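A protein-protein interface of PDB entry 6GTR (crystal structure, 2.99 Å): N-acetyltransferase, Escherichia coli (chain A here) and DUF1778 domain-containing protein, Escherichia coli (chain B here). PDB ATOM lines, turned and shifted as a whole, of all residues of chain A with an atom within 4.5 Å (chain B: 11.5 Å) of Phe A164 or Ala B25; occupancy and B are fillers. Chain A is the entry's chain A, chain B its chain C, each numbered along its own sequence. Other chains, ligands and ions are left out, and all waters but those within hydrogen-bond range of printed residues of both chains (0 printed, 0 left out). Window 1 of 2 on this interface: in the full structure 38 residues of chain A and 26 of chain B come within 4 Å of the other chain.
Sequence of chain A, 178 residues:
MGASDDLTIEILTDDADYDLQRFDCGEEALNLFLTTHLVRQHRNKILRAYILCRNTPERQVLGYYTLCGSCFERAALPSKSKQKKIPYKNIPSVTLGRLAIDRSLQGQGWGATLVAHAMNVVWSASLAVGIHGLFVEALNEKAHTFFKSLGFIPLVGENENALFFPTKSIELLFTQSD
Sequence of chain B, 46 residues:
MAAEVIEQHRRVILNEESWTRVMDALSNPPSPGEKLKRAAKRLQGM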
ATOM      1  N   HIS A 132     -16.995  -8.416   5.278  1.00  0.00           N
ATOM      2  CA  HIS A 132     -17.987  -8.366   4.207  1.00  0.00           C
ATOM      3  C   HIS A 132     -19.321  -7.683   4.498  1.00  0.00           C
ATOM      4  O   HIS A 132     -20.063  -7.384   3.546  1.00  0.00           O
ATOM      5  CB  HIS A 132     -18.227  -9.766   3.674  1.00  0.00           C
ATOM      6  CG  HIS A 132     -17.054 -10.249   2.880  1.00  0.00           C
ATOM      7  ND1 HIS A 132     -16.809  -9.779   1.602  1.00  0.00           N
ATOM      8  CD2 HIS A 132     -16.047 -11.070   3.243  1.00  0.00           C
ATOM      9  CE1 HIS A 132     -15.691 -10.364   1.216  1.00  0.00           C
ATOM     10  NE2 HIS A 132     -15.192 -11.142   2.172  1.00  0.00           N
ATOM     11  N   GLY A 133     -19.706  -7.588   5.763  1.00  0.00           N
ATOM     12  CA  GLY A 133     -20.985  -6.999   6.096  1.00  0.00           C
ATOM     13  C   GLY A 133     -21.191  -6.632   7.546  1.00  0.00           C
ATOM     14  O   GLY A 133     -20.380  -6.964   8.398  1.00  0.00           O
ATOM     15  N   LEU A 134     -22.286  -5.929   7.811  1.00  0.00           N
ATOM     16  CA  LEU A 134     -22.649  -5.539   9.165  1.00  0.00           C
ATOM     17  C   LEU A 134     -23.966  -6.209   9.554  1.00  0.00           C
ATOM     18  O   LEU A 134     -24.954  -6.114   8.835  1.00  0.00           O
ATOM     19  CB  LEU A 134     -22.776  -4.021   9.266  1.00  0.00           C
ATOM     20  CG  LEU A 134     -23.355  -3.455  10.561  1.00  0.00           C
ATOM     21  CD1 LEU A 134     -22.544  -3.911  11.760  1.00  0.00           C
ATOM     22  CD2 LEU A 134     -23.410  -1.940  10.499  1.00  0.00           C
ATOM     23  N   PHE A 135     -23.963  -6.884  10.697  1.00  0.00           N
ATOM     24  CA  PHE A 135     -25.132  -7.582  11.223  1.00  0.00           C
ATOM     25  C   PHE A 135     -25.588  -6.808  12.424  1.00  0.00           C
ATOM     26  O   PHE A 135     -24.783  -6.153  13.091  1.00  0.00           O
ATOM     27  CB  PHE A 135     -24.829  -9.045  11.581  1.00  0.00           C
ATOM     28  CG  PHE A 135     -24.797  -9.979  10.400  1.00  0.00           C
ATOM     29  CD1 PHE A 135     -25.964 -10.576   9.931  1.00  0.00           C
ATOM     30  CD2 PHE A 135     -23.606 -10.250   9.738  1.00  0.00           C
ATOM     31  CE1 PHE A 135     -25.935 -11.449   8.830  1.00  0.00           C
ATOM     32  CE2 PHE A 135     -23.578 -11.129   8.640  1.00  0.00           C
ATOM     33  CZ  PHE A 135     -24.743 -11.725   8.198  1.00  0.00           C
ATOM     34  N   PHE A 152     -31.433  -1.961   6.324  1.00  0.00           N
ATOM     35  CA  PHE A 152     -30.959  -3.270   6.781  1.00  0.00           C
ATOM     36  C   PHE A 152     -31.906  -4.354   6.270  1.00  0.00           C
ATOM     37  O   PHE A 152     -33.123  -4.188   6.343  1.00  0.00           O
ATOM     38  CB  PHE A 152     -30.848  -3.315   8.313  1.00  0.00           C
ATOM     39  CG  PHE A 152     -29.577  -2.718   8.864  1.00  0.00           C
ATOM     40  CD1 PHE A 152     -29.506  -1.369   9.185  1.00  0.00           C
ATOM     41  CD2 PHE A 152     -28.448  -3.501   9.063  1.00  0.00           C
ATOM     42  CE1 PHE A 152     -28.328  -0.816   9.681  1.00  0.00           C
ATOM     43  CE2 PHE A 152     -27.269  -2.942   9.566  1.00  0.00           C
ATOM     44  CZ  PHE A 152     -27.219  -1.606   9.862  1.00  0.00           C
ATOM     45  N   ILE A 153     -31.349  -5.429   5.705  1.00  0.00           N
ATOM     46  CA  ILE A 153     -32.134  -6.530   5.157  1.00  0.00           C
ATOM     47  C   ILE A 153     -32.602  -7.486   6.279  1.00  0.00           C
ATOM     48  O   ILE A 153     -31.763  -8.139   6.911  1.00  0.00           O
ATOM     49  CB  ILE A 153     -31.384  -7.240   3.981  1.00  0.00           C
ATOM     50  CG1 ILE A 153     -31.490  -6.412   2.687  1.00  0.00           C
ATOM     51  CG2 ILE A 153     -31.882  -8.665   3.735  1.00  0.00           C
ATOM     52  CD1 ILE A 153     -30.340  -5.511   2.422  1.00  0.00           C
ATOM     53  N   LEU A 163     -30.569  -8.528  11.096  1.00  0.00           N
ATOM     54  CA  LEU A 163     -30.676  -7.787   9.840  1.00  0.00           C
ATOM     55  C   LEU A 163     -29.255  -7.524   9.359  1.00  0.00           C
ATOM     56  O   LEU A 163     -28.352  -7.375  10.189  1.00  0.00           O
ATOM     57  CB  LEU A 163     -31.419  -6.458  10.013  1.00  0.00           C
ATOM     58  CG  LEU A 163     -32.855  -6.518  10.476  1.00  0.00           C
ATOM     59  CD1 LEU A 163     -32.947  -6.180  11.958  1.00  0.00           C
ATOM     60  CD2 LEU A 163     -33.708  -5.573   9.657  1.00  0.00           C
ATOM     61  N   PHE A 164     -29.052  -7.455   8.031  1.00  0.00           N
ATOM     62  CA  PHE A 164     -27.725  -7.284   7.449  1.00  0.00           C
ATOM     63  C   PHE A 164     -27.593  -6.119   6.488  1.00  0.00           C
ATOM     64  O   PHE A 164     -28.468  -5.895   5.649  1.00  0.00           O
ATOM     65  CB  PHE A 164     -27.322  -8.596   6.758  1.00  0.00           C
ATOM     66  CG  PHE A 164     -26.068  -8.596   5.915  1.00  0.00           C
ATOM     67  CD1 PHE A 164     -24.815  -8.728   6.503  1.00  0.00           C
ATOM     68  CD2 PHE A 164     -26.143  -8.563   4.527  1.00  0.00           C
ATOM     69  CE1 PHE A 164     -23.661  -8.824   5.719  1.00  0.00           C
ATOM     70  CE2 PHE A 164     -24.987  -8.602   3.746  1.00  0.00           C
ATOM     71  CZ  PHE A 164     -23.753  -8.737   4.346  1.00  0.00           C
ATOM     72  N   PHE A 165     -26.452  -5.429   6.561  1.00  0.00           N
ATOM     73  CA  PHE A 165     -26.099  -4.372   5.617  1.00  0.00           C
ATOM     74  C   PHE A 165     -24.718  -4.703   5.033  1.00  0.00           C
ATOM     75  O   PHE A 165     -23.770  -4.841   5.808  1.00  0.00           O
ATOM     76  CB  PHE A 165     -26.050  -3.019   6.293  1.00  0.00           C
ATOM     77  CG  PHE A 165     -26.352  -1.862   5.382  1.00  0.00           C
ATOM     78  CD1 PHE A 165     -27.624  -1.690   4.848  1.00  0.00           C
ATOM     79  CD2 PHE A 165     -25.396  -0.886   5.137  1.00  0.00           C
ATOM     80  CE1 PHE A 165     -27.917  -0.585   4.049  1.00  0.00           C
ATOM     81  CE2 PHE A 165     -25.699   0.233   4.359  1.00  0.00           C
ATOM     82  CZ  PHE A 165     -26.952   0.371   3.816  1.00  0.00           C
ATOM     83  N   PRO A 166     -24.577  -4.876   3.688  1.00  0.00           N
ATOM     84  CA  PRO A 166     -23.256  -5.197   3.125  1.00  0.00           C
ATOM     85  C   PRO A 166     -22.268  -4.051   3.271  1.00  0.00           C
ATOM     86  O   PRO A 166     -22.685  -2.890   3.345  1.00  0.00           O
ATOM     87  CB  PRO A 166     -23.552  -5.441   1.633  1.00  0.00           C
ATOM     88  CG  PRO A 166     -25.005  -5.569   1.529  1.00  0.00           C
ATOM     89  CD  PRO A 166     -25.589  -4.759   2.618  1.00  0.00           C
ATOM     90  N   HIS B   9     -24.264 -13.204  19.574  1.00  0.00           N
ATOM     91  CA  HIS B   9     -24.363 -12.912  18.132  1.00  0.00           C
ATOM     92  C   HIS B   9     -23.000 -12.870  17.370  1.00  0.00           C
ATOM     93  O   HIS B   9     -22.900 -12.241  16.311  1.00  0.00           O
ATOM     94  CB  HIS B   9     -25.090 -11.581  17.930  1.00  0.00           C
ATOM     95  N   VAL B  12     -23.353 -16.326  13.667  1.00  0.00           N
ATOM     96  CA  VAL B  12     -24.614 -16.280  12.976  1.00  0.00           C
ATOM     97  C   VAL B  12     -24.738 -17.593  12.181  1.00  0.00           C
ATOM     98  O   VAL B  12     -24.070 -17.777  11.181  1.00  0.00           O
ATOM     99  CB  VAL B  12     -24.689 -15.030  12.032  1.00  0.00           C
ATOM    100  CG1 VAL B  12     -24.466 -13.743  12.785  1.00  0.00           C
ATOM    101  CG2 VAL B  12     -23.652 -15.122  10.922  1.00  0.00           C
ATOM    102  N   LEU B  14     -27.069 -19.109   9.951  1.00  0.00           N
ATOM    103  CA  LEU B  14     -28.165 -18.769   9.027  1.00  0.00           C
ATOM    104  C   LEU B  14     -28.918 -19.939   8.351  1.00  0.00           C
ATOM    105  O   LEU B  14     -28.315 -20.805   7.703  1.00  0.00           O
ATOM    106  CB  LEU B  14     -27.680 -17.793   7.915  1.00  0.00           C
ATOM    107  CG  LEU B  14     -26.895 -16.529   8.325  1.00  0.00           C
ATOM    108  CD1 LEU B  14     -26.397 -15.787   7.118  1.00  0.00           C
ATOM    109  CD2 LEU B  14     -27.726 -15.601   9.171  1.00  0.00           C
ATOM    110  N   ASN B  15     -30.266 -19.887   8.428  1.00  0.00           N
ATOM    111  CA  ASN B  15     -31.150 -20.827   7.736  1.00  0.00           C
ATOM    112  C   ASN B  15     -31.062 -20.497   6.231  1.00  0.00           C
ATOM    113  O   ASN B  15     -30.761 -19.352   5.863  1.00  0.00           O
ATOM    114  CB  ASN B  15     -32.596 -20.730   8.258  1.00  0.00           C
ATOM    115  CG  ASN B  15     -33.196 -19.342   8.245  1.00  0.00           C
ATOM    116  OD1 ASN B  15     -33.357 -18.703   7.201  1.00  0.00           O
ATOM    117  ND2 ASN B  15     -33.567 -18.851   9.412  1.00  0.00           N
ATOM    118  N   GLU B  16     -31.317 -21.485   5.373  1.00  0.00           N
ATOM    119  CA  GLU B  16     -31.200 -21.355   3.923  1.00  0.00           C
ATOM    120  C   GLU B  16     -31.801 -20.064   3.345  1.00  0.00           C
ATOM    121  O   GLU B  16     -31.151 -19.455   2.497  1.00  0.00           O
ATOM    122  CB  GLU B  16     -31.759 -22.595   3.220  1.00  0.00           C
ATOM    123  CG  GLU B  16     -31.239 -22.796   1.804  1.00  0.00           C
ATOM    124  CD  GLU B  16     -29.740 -22.687   1.584  1.00  0.00           C
ATOM    125  OE1 GLU B  16     -29.338 -22.012   0.605  1.00  0.00           O
ATOM    126  OE2 GLU B  16     -28.969 -23.273   2.381  1.00  0.00           O
ATOM    127  N   GLU B  17     -32.986 -19.624   3.814  1.00  0.00           N
ATOM    128  CA  GLU B  17     -33.618 -18.386   3.312  1.00  0.00           C
ATOM    129  C   GLU B  17     -32.852 -17.131   3.763  1.00  0.00           C
ATOM    130  O   GLU B  17     -32.562 -16.275   2.929  1.00  0.00           O
ATOM    131  CB  GLU B  17     -35.125 -18.313   3.672  1.00  0.00           C
ATOM    132  CG  GLU B  17     -35.830 -16.992   3.359  1.00  0.00           C
ATOM    133  CD  GLU B  17     -36.229 -16.684   1.926  1.00  0.00           C
ATOM    134  OE1 GLU B  17     -37.041 -15.748   1.733  1.00  0.00           O
ATOM    135  OE2 GLU B  17     -35.735 -17.367   0.998  1.00  0.00           O
ATOM    136  N   SER B  18     -32.492 -17.048   5.063  1.00  0.00           N
ATOM    137  CA  SER B  18     -31.719 -15.929   5.596  1.00  0.00           C
ATOM    138  C   SER B  18     -30.365 -15.839   4.887  1.00  0.00           C
ATOM    139  O   SER B  18     -29.903 -14.736   4.588  1.00  0.00           O
ATOM    140  CB  SER B  18     -31.537 -16.073   7.099  1.00  0.00           C
ATOM    141  OG  SER B  18     -32.791 -15.911   7.737  1.00  0.00           O
ATOM    142  N   TRP B  19     -29.776 -17.010   4.557  1.00  0.00           N
ATOM    143  CA  TRP B  19     -28.504 -17.134   3.846  1.00  0.00           C
ATOM    144  C   TRP B  19     -28.583 -16.462   2.476  1.00  0.00           C
ATOM    145  O   TRP B  19     -27.742 -15.604   2.197  1.00  0.00           O
ATOM    146  CB  TRP B  19     -28.088 -18.609   3.719  1.00  0.00           C
ATOM    147  CG  TRP B  19     -26.857 -18.827   2.889  1.00  0.00           C
ATOM    148  CD1 TRP B  19     -26.802 -19.318   1.617  1.00  0.00           C
ATOM    149  CD2 TRP B  19     -25.508 -18.528   3.262  1.00  0.00           C
ATOM    150  NE1 TRP B  19     -25.498 -19.362   1.182  1.00  0.00           N
ATOM    151  CE2 TRP B  19     -24.681 -18.891   2.176  1.00  0.00           C
ATOM    152  CE3 TRP B  19     -24.907 -18.026   4.429  1.00  0.00           C
ATOM    153  CZ2 TRP B  19     -23.292 -18.748   2.215  1.00  0.00           C
ATOM    154  CZ3 TRP B  19     -23.528 -17.890   4.469  1.00  0.00           C
ATOM    155  CH2 TRP B  19     -22.736 -18.258   3.376  1.00  0.00           C
ATOM    156  N   THR B  20     -29.606 -16.825   1.651  1.00  0.00           N
ATOM    157  CA  THR B  20     -29.810 -16.286   0.296  1.00  0.00           C
ATOM    158  C   THR B  20     -29.993 -14.761   0.301  1.00  0.00           C
ATOM    159  O   THR B  20     -29.434 -14.102  -0.574  1.00  0.00           O
ATOM    160  CB  THR B  20     -30.937 -17.004  -0.481  1.00  0.00           C
ATOM    161  OG1 THR B  20     -32.196 -16.757   0.137  1.00  0.00           O
ATOM    162  CG2 THR B  20     -30.703 -18.487  -0.634  1.00  0.00           C
ATOM    163  N   ARG B  21     -30.722 -14.206   1.310  1.00  0.00           N
ATOM    164  CA  ARG B  21     -30.951 -12.769   1.514  1.00  0.00           C
ATOM    165  C   ARG B  21     -29.626 -12.044   1.608  1.00  0.00           C
ATOM    166  O   ARG B  21     -29.453 -11.045   0.917  1.00  0.00           O
ATOM    167  CB  ARG B  21     -31.809 -12.497   2.770  1.00  0.00           C
ATOM    168  CG  ARG B  21     -33.243 -13.005   2.611  1.00  0.00           C
ATOM    169  CD  ARG B  21     -34.290 -12.413   3.524  1.00  0.00           C
ATOM    170  NE  ARG B  21     -35.619 -12.750   3.013  1.00  0.00           N
ATOM    171  CZ  ARG B  21     -36.757 -12.612   3.690  1.00  0.00           C
ATOM    172  NH1 ARG B  21     -36.746 -12.161   4.938  1.00  0.00           N
ATOM    173  NH2 ARG B  21     -37.913 -12.928   3.127  1.00  0.00           N
ATOM    174  N   VAL B  22     -28.669 -12.586   2.397  1.00  0.00           N
ATOM    175  CA  VAL B  22     -27.315 -12.045   2.564  1.00  0.00           C
ATOM    176  C   VAL B  22     -26.541 -12.188   1.232  1.00  0.00           C
ATOM    177  O   VAL B  22     -26.037 -11.197   0.695  1.00  0.00           O
ATOM    178  CB  VAL B  22     -26.564 -12.684   3.767  1.00  0.00           C
ATOM    179  CG1 VAL B  22     -25.115 -12.210   3.823  1.00  0.00           C
ATOM    180  CG2 VAL B  22     -27.266 -12.378   5.092  1.00  0.00           C
ATOM    181  N   MET B  23     -26.490 -13.406   0.680  1.00  0.00           N
ATOM    182  CA  MET B  23     -25.824 -13.668  -0.590  1.00  0.00           C
ATOM    183  C   MET B  23     -26.248 -12.675  -1.652  1.00  0.00           C
ATOM    184  O   MET B  23     -25.395 -12.187  -2.409  1.00  0.00           O
ATOM    185  CB  MET B  23     -26.091 -15.105  -1.047  1.00  0.00           C
ATOM    186  CG  MET B  23     -25.250 -16.121  -0.338  1.00  0.00           C
ATOM    187  SD  MET B  23     -23.516 -15.630  -0.167  1.00  0.00           S
ATOM    188  CE  MET B  23     -23.482 -15.202   1.546  1.00  0.00           C
ATOM    189  N   ASP B  24     -27.570 -12.370  -1.683  1.00  0.00           N
ATOM    190  CA  ASP B  24     -28.218 -11.446  -2.615  1.00  0.00           C
ATOM    191  C   ASP B  24     -27.925 -10.005  -2.269  1.00  0.00           C
ATOM    192  O   ASP B  24     -27.901  -9.165  -3.171  1.00  0.00           O
ATOM    193  CB  ASP B  24     -29.741 -11.664  -2.665  1.00  0.00           C
ATOM    194  CG  ASP B  24     -30.208 -12.956  -3.315  1.00  0.00           C
ATOM    195  OD1 ASP B  24     -29.339 -13.770  -3.728  1.00  0.00           O
ATOM    196  OD2 ASP B  24     -31.444 -13.157  -3.405  1.00  0.00           O
ATOM    197  N   ALA B  25     -27.734  -9.703  -0.973  1.00  0.00           N
ATOM    198  CA  ALA B  25     -27.414  -8.347  -0.553  1.00  0.00           C
ATOM    199  C   ALA B  25     -25.977  -8.022  -1.001  1.00  0.00           C
ATOM    200  O   ALA B  25     -25.708  -6.881  -1.383  1.00  0.00           O
ATOM    201  CB  ALA B  25     -27.579  -8.193   0.949  1.00  0.00           C
ATOM    202  N   LEU B  26     -25.086  -9.048  -1.050  1.00  0.00           N
ATOM    203  CA  LEU B  26     -23.693  -8.880  -1.483  1.00  0.00           C
ATOM    204  C   LEU B  26     -23.571  -8.684  -3.006  1.00  0.00           C
ATOM    205  O   LEU B  26     -22.687  -7.940  -3.453  1.00  0.00           O
ATOM    206  CB  LEU B  26     -22.823 -10.074  -1.045  1.00  0.00           C
ATOM    207  CG  LEU B  26     -22.732 -10.415   0.457  1.00  0.00           C
ATOM    208  CD1 LEU B  26     -22.188 -11.800   0.634  1.00  0.00           C
ATOM    209  CD2 LEU B  26     -21.844  -9.434   1.215  1.00  0.00           C
ATOM    210  N   SER B  27     -24.422  -9.382  -3.804  1.00  0.00           N
ATOM    211  CA  SER B  27     -24.391  -9.309  -5.269  1.00  0.00           C
ATOM    212  C   SER B  27     -25.188  -8.148  -5.780  1.00  0.00           C
ATOM    213  O   SER B  27     -24.850  -7.587  -6.830  1.00  0.00           O
ATOM    214  CB  SER B  27     -24.847 -10.615  -5.902  1.00  0.00           C
ATOM    215  OG  SER B  27     -26.080 -11.056  -5.367  1.00  0.00           O
ATOM    216  N   ASN B  28     -26.218  -7.750  -5.019  1.00  0.00           N
ATOM    217  CA  ASN B  28     -27.068  -6.593  -5.313  1.00  0.00           C
ATOM    218  C   ASN B  28     -27.134  -5.683  -4.081  1.00  0.00           C
ATOM    219  O   ASN B  28     -28.144  -5.658  -3.364  1.00  0.00           O
ATOM    220  CB  ASN B  28     -28.463  -7.016  -5.795  1.00  0.00           C
ATOM    221  CG  ASN B  28     -29.330  -5.856  -6.216  1.00  0.00           C
ATOM    222  OD1 ASN B  28     -28.848  -4.815  -6.704  1.00  0.00           O
ATOM    223  ND2 ASN B  28     -30.632  -6.011  -6.027  1.00  0.00           N
ATOM    224  N   PRO B  29     -26.046  -4.957  -3.783  1.00  0.00           N
ATOM    225  CA  PRO B  29     -26.046  -4.133  -2.568  1.00  0.00           C
ATOM    226  C   PRO B  29     -27.059  -3.005  -2.561  1.00  0.00           C
ATOM    227  O   PRO B  29     -27.083  -2.195  -3.496  1.00  0.00           O
ATOM    228  CB  PRO B  29     -24.599  -3.620  -2.475  1.00  0.00           C
ATOM    229  CG  PRO B  29     -23.807  -4.496  -3.393  1.00  0.00           C
ATOM    230  CD  PRO B  29     -24.754  -4.870  -4.485  1.00  0.00           C
ATOM    231  N   PRO B  30     -27.891  -2.928  -1.503  1.00  0.00           N
ATOM    232  CA  PRO B  30     -28.862  -1.823  -1.395  1.00  0.00           C
ATOM    233  C   PRO B  30     -28.278  -0.426  -1.576  1.00  0.00           C
ATOM    234  O   PRO B  30     -27.164  -0.163  -1.148  1.00  0.00           O
ATOM    235  CB  PRO B  30     -29.399  -1.961   0.033  1.00  0.00           C
ATOM    236  CG  PRO B  30     -28.491  -2.913   0.726  1.00  0.00           C
ATOM    237  CD  PRO B  30     -27.989  -3.826  -0.340  1.00  0.00           C
ATOM    238  N   SER B  31     -29.030   0.469  -2.222  1.00  0.00           N
ATOM    239  CA  SER B  31     -28.604   1.848  -2.406  1.00  0.00           C
ATOM    240  C   SER B  31     -28.978   2.577  -1.125  1.00  0.00           C
ATOM    241  O   SER B  31     -30.134   2.447  -0.695  1.00  0.00           O
ATOM    242  CB  SER B  31     -29.326   2.477  -3.586  1.00  0.00           C
ATOM    243  OG  SER B  31     -28.927   1.863  -4.799  1.00  0.00           O
ATOM    244  N   PRO B  32     -28.024   3.287  -0.454  1.00  0.00           N
ATOM    245  CA  PRO B  32     -28.374   3.995   0.790  1.00  0.00           C
ATOM    246  C   PRO B  32     -29.569   4.939   0.631  1.00  0.00           C
ATOM    247  O   PRO B  32     -29.622   5.746  -0.313  1.00  0.00           O
ATOM    248  CB  PRO B  32     -27.088   4.734   1.148  1.00  0.00           C
ATOM    249  CG  PRO B  32     -26.013   3.909   0.515  1.00  0.00           C
ATOM    250  CD  PRO B  32     -26.603   3.494  -0.791  1.00  0.00           C
ATOM    251  N   LEU B  36     -30.629   7.288   5.934  1.00  0.00           N
ATOM    252  CA  LEU B  36     -29.233   6.930   6.212  1.00  0.00           C
ATOM    253  C   LEU B  36     -28.248   8.008   5.763  1.00  0.00           C
ATOM    254  O   LEU B  36     -27.334   8.342   6.519  1.00  0.00           O
ATOM    255  CB  LEU B  36     -28.879   5.564   5.615  1.00  0.00           C
ATOM    256  CG  LEU B  36     -27.592   4.916   6.122  1.00  0.00           C
ATOM    257  CD1 LEU B  36     -27.656   4.644   7.600  1.00  0.00           C
ATOM    258  CD2 LEU B  36     -27.307   3.634   5.381  1.00  0.00           C
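The backbone carbonyl oxygen (O) of Phe A164 lies within hydrogen-bond range of the backbone NH (N) of Ile A153 (2.9 Å). The backbone NH (N) of Leu A134 lies within hydrogen-bond range of the backbone carbonyl oxygen (O) of Phe A165, 2.7 Å away. The side-chain carboxylate (OE1) of Glu B17 is in salt-bridge range of the guanidinium group (NH2) of Arg B21, 3.3 Å away.
CD2 of Leu B26 touches O of His A132, at 3.6 Å. CG2 of Ile A153 touches CB of Arg B21, at 3.95 Å. Pro B30 touches Ile A153 (CG to CD1, 3.6 Å). Phe A164 touches Val B22 (CE2 to CG1, 3.6 Å). CE2 of Phe A164 touches CB of Ala B25 (3.8 Å). Phe A164 touches Leu B26. CZ of Phe A165 touches CD2 of Leu B36, at 3.6 Å. Pro A166 touches Ala B25. CD of Pro A166 touches CD of Pro B30 (3.9 Å).
Of the printed residues of chain B, His A132 touches Leu B26 (3.6 Å). No residue of chain B comes within 4 Å of Gly A133. No residue of chain B comes within 4 Å of Phe A135. Of chain B, only Arg B21 and Pro B30 come within 4 Å of Ile A153. No residue of chain B comes within 4 Å of Leu A163. Val B12 touches none of the printed residues of chain A. Of the printed residues of chain A, Val B22 touches Phe A164. Of chain A, only Phe A164 (3.8 Å) and Pro A166 (3.3 Å) come within 4 Å of Ala B25. Pro B32 touches none of the printed residues of chain A. Printed residues of chain A within 4 Å of Leu B36: Phe A165. The nearest printed residue of chain A that does not touch Val B22 is Phe A135 (4.1 Å).
Hydrophobic or aromatic side chains of chain B that line the printed part of chain A: Val B22, Ala B25, Leu B26, Pro B30 and Leu B36. Hydrophobic or aromatic side chains of chain A that line the printed part of chain B: Ile A153, Phe A164, Phe A165 and Pro A166. Among the printed residues, 9 pairs touch across the chains.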
